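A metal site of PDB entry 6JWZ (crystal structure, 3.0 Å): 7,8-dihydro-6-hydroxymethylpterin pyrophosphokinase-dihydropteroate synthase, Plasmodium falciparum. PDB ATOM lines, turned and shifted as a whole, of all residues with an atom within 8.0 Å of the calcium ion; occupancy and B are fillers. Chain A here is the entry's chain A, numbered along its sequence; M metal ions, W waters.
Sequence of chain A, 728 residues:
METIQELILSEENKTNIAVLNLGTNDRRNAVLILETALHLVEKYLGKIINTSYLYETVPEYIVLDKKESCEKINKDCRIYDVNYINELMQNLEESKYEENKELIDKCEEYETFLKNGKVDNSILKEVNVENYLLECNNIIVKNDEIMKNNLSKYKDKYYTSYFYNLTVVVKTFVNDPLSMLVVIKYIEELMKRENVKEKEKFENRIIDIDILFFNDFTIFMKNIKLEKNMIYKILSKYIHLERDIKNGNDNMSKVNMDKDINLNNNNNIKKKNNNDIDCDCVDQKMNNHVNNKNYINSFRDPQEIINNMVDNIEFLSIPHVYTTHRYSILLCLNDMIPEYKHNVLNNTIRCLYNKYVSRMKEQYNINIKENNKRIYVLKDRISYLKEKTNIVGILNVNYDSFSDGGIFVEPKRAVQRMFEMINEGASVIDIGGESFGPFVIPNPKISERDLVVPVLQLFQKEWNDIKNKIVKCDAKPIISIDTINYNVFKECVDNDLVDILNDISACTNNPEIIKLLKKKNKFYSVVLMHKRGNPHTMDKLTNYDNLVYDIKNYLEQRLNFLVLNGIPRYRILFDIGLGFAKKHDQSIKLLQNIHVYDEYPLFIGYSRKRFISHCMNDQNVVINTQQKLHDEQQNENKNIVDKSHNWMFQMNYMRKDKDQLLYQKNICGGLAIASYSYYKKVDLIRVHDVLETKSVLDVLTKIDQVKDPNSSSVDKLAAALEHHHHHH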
ATOM      1  N   LEU A  38     -12.772  22.503 -25.784  1.00  0.00           N
ATOM      2  CA  LEU A  38     -13.359  21.739 -24.682  1.00  0.00           C
ATOM      3  C   LEU A  38     -14.066  22.691 -23.712  1.00  0.00           C
ATOM      4  O   LEU A  38     -15.165  22.379 -23.233  1.00  0.00           O
ATOM      5  CB  LEU A  38     -12.253  20.969 -23.962  1.00  0.00           C
ATOM      6  CG  LEU A  38     -11.989  19.534 -24.442  1.00  0.00           C
ATOM      7  CD1 LEU A  38     -10.844  18.920 -23.659  1.00  0.00           C
ATOM      8  CD2 LEU A  38     -13.232  18.680 -24.292  1.00  0.00           C
ATOM      9  N   HIS A  39     -13.427  23.842 -23.452  1.00  0.00           N
ATOM     10  CA  HIS A  39     -13.952  24.860 -22.556  1.00  0.00           C
ATOM     11  C   HIS A  39     -15.242  25.466 -23.090  1.00  0.00           C
ATOM     12  O   HIS A  39     -16.276  25.442 -22.412  1.00  0.00           O
ATOM     13  CB  HIS A  39     -12.888  25.919 -22.282  1.00  0.00           C
ATOM     14  CG  HIS A  39     -11.896  25.478 -21.267  1.00  0.00           C
ATOM     15  ND1 HIS A  39     -10.543  25.441 -21.528  1.00  0.00           N
ATOM     16  CD2 HIS A  39     -12.061  25.033 -20.008  1.00  0.00           C
ATOM     17  CE1 HIS A  39      -9.913  24.992 -20.467  1.00  0.00           C
ATOM     18  NE2 HIS A  39     -10.809  24.762 -19.512  1.00  0.00           N
ATOM     19  N   LEU A  40     -15.205  25.999 -24.317  1.00  0.00           N
ATOM     20  CA  LEU A  40     -16.403  26.573 -24.913  1.00  0.00           C
ATOM     21  C   LEU A  40     -17.490  25.518 -25.050  1.00  0.00           C
ATOM     22  O   LEU A  40     -18.661  25.839 -25.083  1.00  0.00           O
ATOM     23  CB  LEU A  40     -16.066  27.235 -26.249  1.00  0.00           C
ATOM     24  CG  LEU A  40     -15.083  28.394 -26.155  1.00  0.00           C
ATOM     25  CD1 LEU A  40     -14.541  28.791 -27.528  1.00  0.00           C
ATOM     26  CD2 LEU A  40     -15.720  29.572 -25.439  1.00  0.00           C
ATOM     27  N   VAL A  41     -17.096  24.236 -25.090  1.00  0.00           N
ATOM     28  CA  VAL A  41     -18.105  23.186 -25.072  1.00  0.00           C
ATOM     29  C   VAL A  41     -18.791  23.205 -23.712  1.00  0.00           C
ATOM     30  O   VAL A  41     -20.017  23.239 -23.661  1.00  0.00           O
ATOM     31  CB  VAL A  41     -17.545  21.796 -25.412  1.00  0.00           C
ATOM     32  CG1 VAL A  41     -18.590  20.708 -25.193  1.00  0.00           C
ATOM     33  CG2 VAL A  41     -16.987  21.734 -26.829  1.00  0.00           C
ATOM     34  N   GLU A  42     -17.986  23.184 -22.627  1.00  0.00           N
ATOM     35  CA  GLU A  42     -18.502  23.103 -21.262  1.00  0.00           C
ATOM     36  C   GLU A  42     -19.319  24.347 -20.944  1.00  0.00           C
ATOM     37  O   GLU A  42     -20.274  24.276 -20.164  1.00  0.00           O
ATOM     38  CB  GLU A  42     -17.366  23.084 -20.235  1.00  0.00           C
ATOM     39  CG  GLU A  42     -17.155  21.740 -19.585  1.00  0.00           C
ATOM     40  CD  GLU A  42     -18.220  21.263 -18.611  1.00  0.00           C
ATOM     41  OE1 GLU A  42     -19.102  22.068 -18.237  1.00  0.00           O
ATOM     42  OE2 GLU A  42     -18.173  20.059 -18.231  1.00  0.00           O
ATOM     43  N   LYS A  43     -18.905  25.474 -21.532  1.00  0.00           N
ATOM     44  CA  LYS A  43     -19.519  26.771 -21.282  1.00  0.00           C
ATOM     45  C   LYS A  43     -20.907  26.819 -21.919  1.00  0.00           C
ATOM     46  O   LYS A  43     -21.857  27.212 -21.236  1.00  0.00           O
ATOM     47  CB  LYS A  43     -18.642  27.869 -21.877  1.00  0.00           C
ATOM     48  CG  LYS A  43     -19.183  29.286 -21.724  1.00  0.00           C
ATOM     49  CD  LYS A  43     -18.115  30.352 -21.933  1.00  0.00           C
ATOM     50  CE  LYS A  43     -18.419  31.633 -21.176  1.00  0.00           C
ATOM     51  NZ  LYS A  43     -19.018  31.355 -19.850  1.00  0.00           N
ATOM     52  N   TYR A  44     -20.991  26.378 -23.177  1.00  0.00           N
ATOM     53  CA  TYR A  44     -22.086  26.707 -24.080  1.00  0.00           C
ATOM     54  C   TYR A  44     -22.960  25.515 -24.472  1.00  0.00           C
ATOM     55  O   TYR A  44     -24.045  25.732 -24.989  1.00  0.00           O
ATOM     56  CB  TYR A  44     -21.538  27.323 -25.365  1.00  0.00           C
ATOM     57  CG  TYR A  44     -21.004  28.719 -25.218  1.00  0.00           C
ATOM     58  CD1 TYR A  44     -21.708  29.682 -24.523  1.00  0.00           C
ATOM     59  CD2 TYR A  44     -19.806  29.085 -25.824  1.00  0.00           C
ATOM     60  CE1 TYR A  44     -21.229  30.984 -24.401  1.00  0.00           C
ATOM     61  CE2 TYR A  44     -19.312  30.377 -25.713  1.00  0.00           C
ATOM     62  CZ  TYR A  44     -20.021  31.325 -24.993  1.00  0.00           C
ATOM     63  OH  TYR A  44     -19.540  32.598 -24.863  1.00  0.00           O
ATOM     64  N   LEU A  45     -22.503  24.270 -24.285  1.00  0.00           N
ATOM     65  CA  LEU A  45     -23.299  23.138 -24.756  1.00  0.00           C
ATOM     66  C   LEU A  45     -23.883  22.344 -23.580  1.00  0.00           C
ATOM     67  O   LEU A  45     -24.959  21.756 -23.680  1.00  0.00           O
ATOM     68  CB  LEU A  45     -22.494  22.254 -25.714  1.00  0.00           C
ATOM     69  CG  LEU A  45     -22.005  22.916 -27.004  1.00  0.00           C
ATOM     70  CD1 LEU A  45     -21.016  22.050 -27.749  1.00  0.00           C
ATOM     71  CD2 LEU A  45     -23.171  23.243 -27.927  1.00  0.00           C
ATOM     72  N   GLY A  46     -23.170  22.355 -22.435  1.00  0.00           N
ATOM     73  CA  GLY A  46     -23.572  21.554 -21.291  1.00  0.00           C
ATOM     74  C   GLY A  46     -22.359  21.017 -20.548  1.00  0.00           C
ATOM     75  O   GLY A  46     -21.368  21.724 -20.387  1.00  0.00           O
ATOM     76  N   LYS A  47     -22.429  19.743 -20.170  1.00  0.00           N
ATOM     77  CA  LYS A  47     -21.455  19.140 -19.266  1.00  0.00           C
ATOM     78  C   LYS A  47     -20.715  17.991 -19.957  1.00  0.00           C
ATOM     79  O   LYS A  47     -21.350  17.071 -20.461  1.00  0.00           O
ATOM     80  CB  LYS A  47     -22.179  18.657 -18.011  1.00  0.00           C
ATOM     81  CG  LYS A  47     -21.420  17.638 -17.193  1.00  0.00           C
ATOM     82  CD  LYS A  47     -21.549  17.849 -15.718  1.00  0.00           C
ATOM     83  CE  LYS A  47     -20.322  17.404 -14.970  1.00  0.00           C
ATOM     84  NZ  LYS A  47     -20.658  17.101 -13.566  1.00  0.00           N
ATOM     85  N   ILE A  48     -19.377  18.049 -19.961  1.00  0.00           N
ATOM     86  CA  ILE A  48     -18.549  16.953 -20.460  1.00  0.00           C
ATOM     87  C   ILE A  48     -18.551  15.803 -19.450  1.00  0.00           C
ATOM     88  O   ILE A  48     -18.244  16.004 -18.285  1.00  0.00           O
ATOM     89  CB  ILE A  48     -17.113  17.436 -20.725  1.00  0.00           C
ATOM     90  CG1 ILE A  48     -17.068  18.385 -21.918  1.00  0.00           C
ATOM     91  CG2 ILE A  48     -16.206  16.231 -20.925  1.00  0.00           C
ATOM     92  CD1 ILE A  48     -15.820  19.221 -21.994  1.00  0.00           C
ATOM     93  N   SER A  95     -23.101  32.442 -20.654  1.00  0.00           N
ATOM     94  CA  SER A  95     -24.086  31.459 -21.090  1.00  0.00           C
ATOM     95  C   SER A  95     -25.390  31.710 -20.352  1.00  0.00           C
ATOM     96  O   SER A  95     -25.391  32.043 -19.166  1.00  0.00           O
ATOM     97  CB  SER A  95     -23.603  30.051 -20.846  1.00  0.00           C
ATOM     98  OG  SER A  95     -24.679  29.132 -20.873  1.00  0.00           O
ATOM     99  N   TYR A  97     -27.179  29.451 -19.635  1.00  0.00           N
ATOM    100  CA  TYR A  97     -27.324  28.207 -18.879  1.00  0.00           C
ATOM    101  C   TYR A  97     -26.234  28.120 -17.810  1.00  0.00           C
ATOM    102  O   TYR A  97     -25.125  28.607 -17.990  1.00  0.00           O
ATOM    103  CB  TYR A  97     -27.379  27.003 -19.817  1.00  0.00           C
ATOM    104  CG  TYR A  97     -28.744  26.727 -20.403  1.00  0.00           C
ATOM    105  CD1 TYR A  97     -29.190  27.418 -21.523  1.00  0.00           C
ATOM    106  CD2 TYR A  97     -29.596  25.792 -19.836  1.00  0.00           C
ATOM    107  CE1 TYR A  97     -30.447  27.192 -22.072  1.00  0.00           C
ATOM    108  CE2 TYR A  97     -30.854  25.543 -20.381  1.00  0.00           C
ATOM    109  CZ  TYR A  97     -31.280  26.243 -21.499  1.00  0.00           C
ATOM    110  OH  TYR A  97     -32.513  26.017 -22.041  1.00  0.00           O
ATOM    111  N   GLU A  98     -26.587  27.503 -16.693  1.00  0.00           N
ATOM    112  CA  GLU A  98     -25.752  27.597 -15.504  1.00  0.00           C
ATOM    113  C   GLU A  98     -24.735  26.459 -15.498  1.00  0.00           C
ATOM    114  O   GLU A  98     -24.981  25.400 -16.072  1.00  0.00           O
ATOM    115  CB  GLU A  98     -26.611  27.527 -14.252  1.00  0.00           C
ATOM    116  CG  GLU A  98     -27.638  26.417 -14.289  1.00  0.00           C
ATOM    117  CD  GLU A  98     -28.348  26.237 -12.970  1.00  0.00           C
ATOM    118  OE1 GLU A  98     -28.201  27.129 -12.099  1.00  0.00           O
ATOM    119  OE2 GLU A  98     -29.033  25.209 -12.809  1.00  0.00           O
ATOM    120  N   GLU A  99     -23.624  26.688 -14.794  1.00  0.00           N
ATOM    121  CA  GLU A  99     -22.505  25.763 -14.711  1.00  0.00           C
ATOM    122  C   GLU A  99     -22.469  25.163 -13.305  1.00  0.00           C
ATOM    123  O   GLU A  99     -22.410  25.902 -12.343  1.00  0.00           O
ATOM    124  CB  GLU A  99     -21.215  26.531 -14.988  1.00  0.00           C
ATOM    125  CG  GLU A  99     -19.987  25.665 -14.986  1.00  0.00           C
ATOM    126  CD  GLU A  99     -19.917  24.716 -16.164  1.00  0.00           C
ATOM    127  OE1 GLU A  99     -20.555  23.632 -16.097  1.00  0.00           O
ATOM    128  OE2 GLU A  99     -19.245  25.055 -17.156  1.00  0.00           O
ATOM    129  N   ASN A 100     -22.466  23.828 -13.183  1.00  0.00           N
ATOM    130  CA  ASN A 100     -22.556  23.199 -11.874  1.00  0.00           C
ATOM    131  C   ASN A 100     -21.410  22.234 -11.616  1.00  0.00           C
ATOM    132  O   ASN A 100     -21.475  21.068 -12.005  1.00  0.00           O
ATOM    133  CB  ASN A 100     -23.899  22.499 -11.656  1.00  0.00           C
ATOM    134  CG  ASN A 100     -25.040  23.478 -11.532  1.00  0.00           C
ATOM    135  OD1 ASN A 100     -24.941  24.498 -10.860  1.00  0.00           O
ATOM    136  ND2 ASN A 100     -26.158  23.162 -12.170  1.00  0.00           N
ATOM    137  N   LYS A 101     -20.404  22.698 -10.866  1.00  0.00           N
ATOM    138  CA  LYS A 101     -19.178  21.954 -10.656  1.00  0.00           C
ATOM    139  C   LYS A 101     -19.312  20.863  -9.597  1.00  0.00           C
ATOM    140  O   LYS A 101     -18.299  20.287  -9.231  1.00  0.00           O
ATOM    141  CB  LYS A 101     -18.005  22.878 -10.354  1.00  0.00           C
ATOM    142  CG  LYS A 101     -17.780  24.008 -11.360  1.00  0.00           C
ATOM    143  CD  LYS A 101     -16.438  24.725 -11.255  1.00  0.00           C
ATOM    144  CE  LYS A 101     -16.517  26.126 -11.848  1.00  0.00           C
ATOM    145  NZ  LYS A 101     -15.225  26.860 -11.854  1.00  0.00           N
ATOM    146  N   VAL A 170     -21.182  14.997 -24.199  1.00  0.00           N
ATOM    147  CA  VAL A 170     -21.708  16.173 -23.522  1.00  0.00           C
ATOM    148  C   VAL A 170     -23.139  15.869 -23.082  1.00  0.00           C
ATOM    149  O   VAL A 170     -23.983  15.640 -23.934  1.00  0.00           O
ATOM    150  CB  VAL A 170     -21.734  17.396 -24.465  1.00  0.00           C
ATOM    151  CG1 VAL A 170     -21.967  18.693 -23.706  1.00  0.00           C
ATOM    152  CG2 VAL A 170     -20.506  17.501 -25.357  1.00  0.00           C
ATOM    153  N   LYS A 171     -23.398  15.848 -21.768  1.00  0.00           N
ATOM    154  CA  LYS A 171     -24.780  16.023 -21.340  1.00  0.00           C
ATOM    155  C   LYS A 171     -25.156  17.439 -21.734  1.00  0.00           C
ATOM    156  O   LYS A 171     -24.482  18.395 -21.350  1.00  0.00           O
ATOM    157  CB  LYS A 171     -24.951  15.803 -19.832  1.00  0.00           C
ATOM    158  CG  LYS A 171     -26.390  15.553 -19.397  1.00  0.00           C
ATOM    159  CD  LYS A 171     -26.576  15.383 -17.900  1.00  0.00           C
ATOM    160  CE  LYS A 171     -25.576  14.460 -17.233  1.00  0.00           C
ATOM    161  NZ  LYS A 171     -25.603  14.545 -15.752  1.00  0.00           N
ATOM    162  N   PHE A 173     -27.953  20.665 -22.867  1.00  0.00           N
ATOM    163  CA  PHE A 173     -29.204  21.358 -22.641  1.00  0.00           C
ATOM    164  C   PHE A 173     -29.746  21.903 -23.964  1.00  0.00           C
ATOM    165  O   PHE A 173     -30.860  22.414 -24.019  1.00  0.00           O
ATOM    166  CB  PHE A 173     -29.047  22.450 -21.583  1.00  0.00           C
ATOM    167  CG  PHE A 173     -27.835  23.334 -21.765  1.00  0.00           C
ATOM    168  CD1 PHE A 173     -27.590  23.969 -22.974  1.00  0.00           C
ATOM    169  CD2 PHE A 173     -26.937  23.515 -20.727  1.00  0.00           C
ATOM    170  CE1 PHE A 173     -26.470  24.769 -23.135  1.00  0.00           C
ATOM    171  CE2 PHE A 173     -25.827  24.326 -20.885  1.00  0.00           C
ATOM    172  CZ  PHE A 173     -25.585  24.947 -22.094  1.00  0.00           C
HETATM  173 CA    CA M   1     -21.235  23.263 -18.384  1.00  0.00          CA
HETATM  174  O   HOH W   1     -22.587  21.736 -17.443  1.00  0.00           O
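The nearest printed residue that does not touch the calcium ion is Lys 47 (4.1 Å).
The calcium ion is bound by water W1, the backbone carbonyl oxygen (O) of Glu 42, the side-chain carboxylate (OE1) of Glu 99, the side-chain carboxylate (OE1) of Glu 42 and the backbone carbonyl oxygen (O) of Gly 46. The calcium ion has five donor atoms within binding distance. Slightly farther from the calcium ion lies the side-chain carboxylate (OE2) of Glu 99 (2.9 Å).
N of Ile 48 lies within hydrogen-bond range of OE2 of Glu 42. O of Val 41 is in hydrogen-bond range of N of Gly 46, at 3.5 Å.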
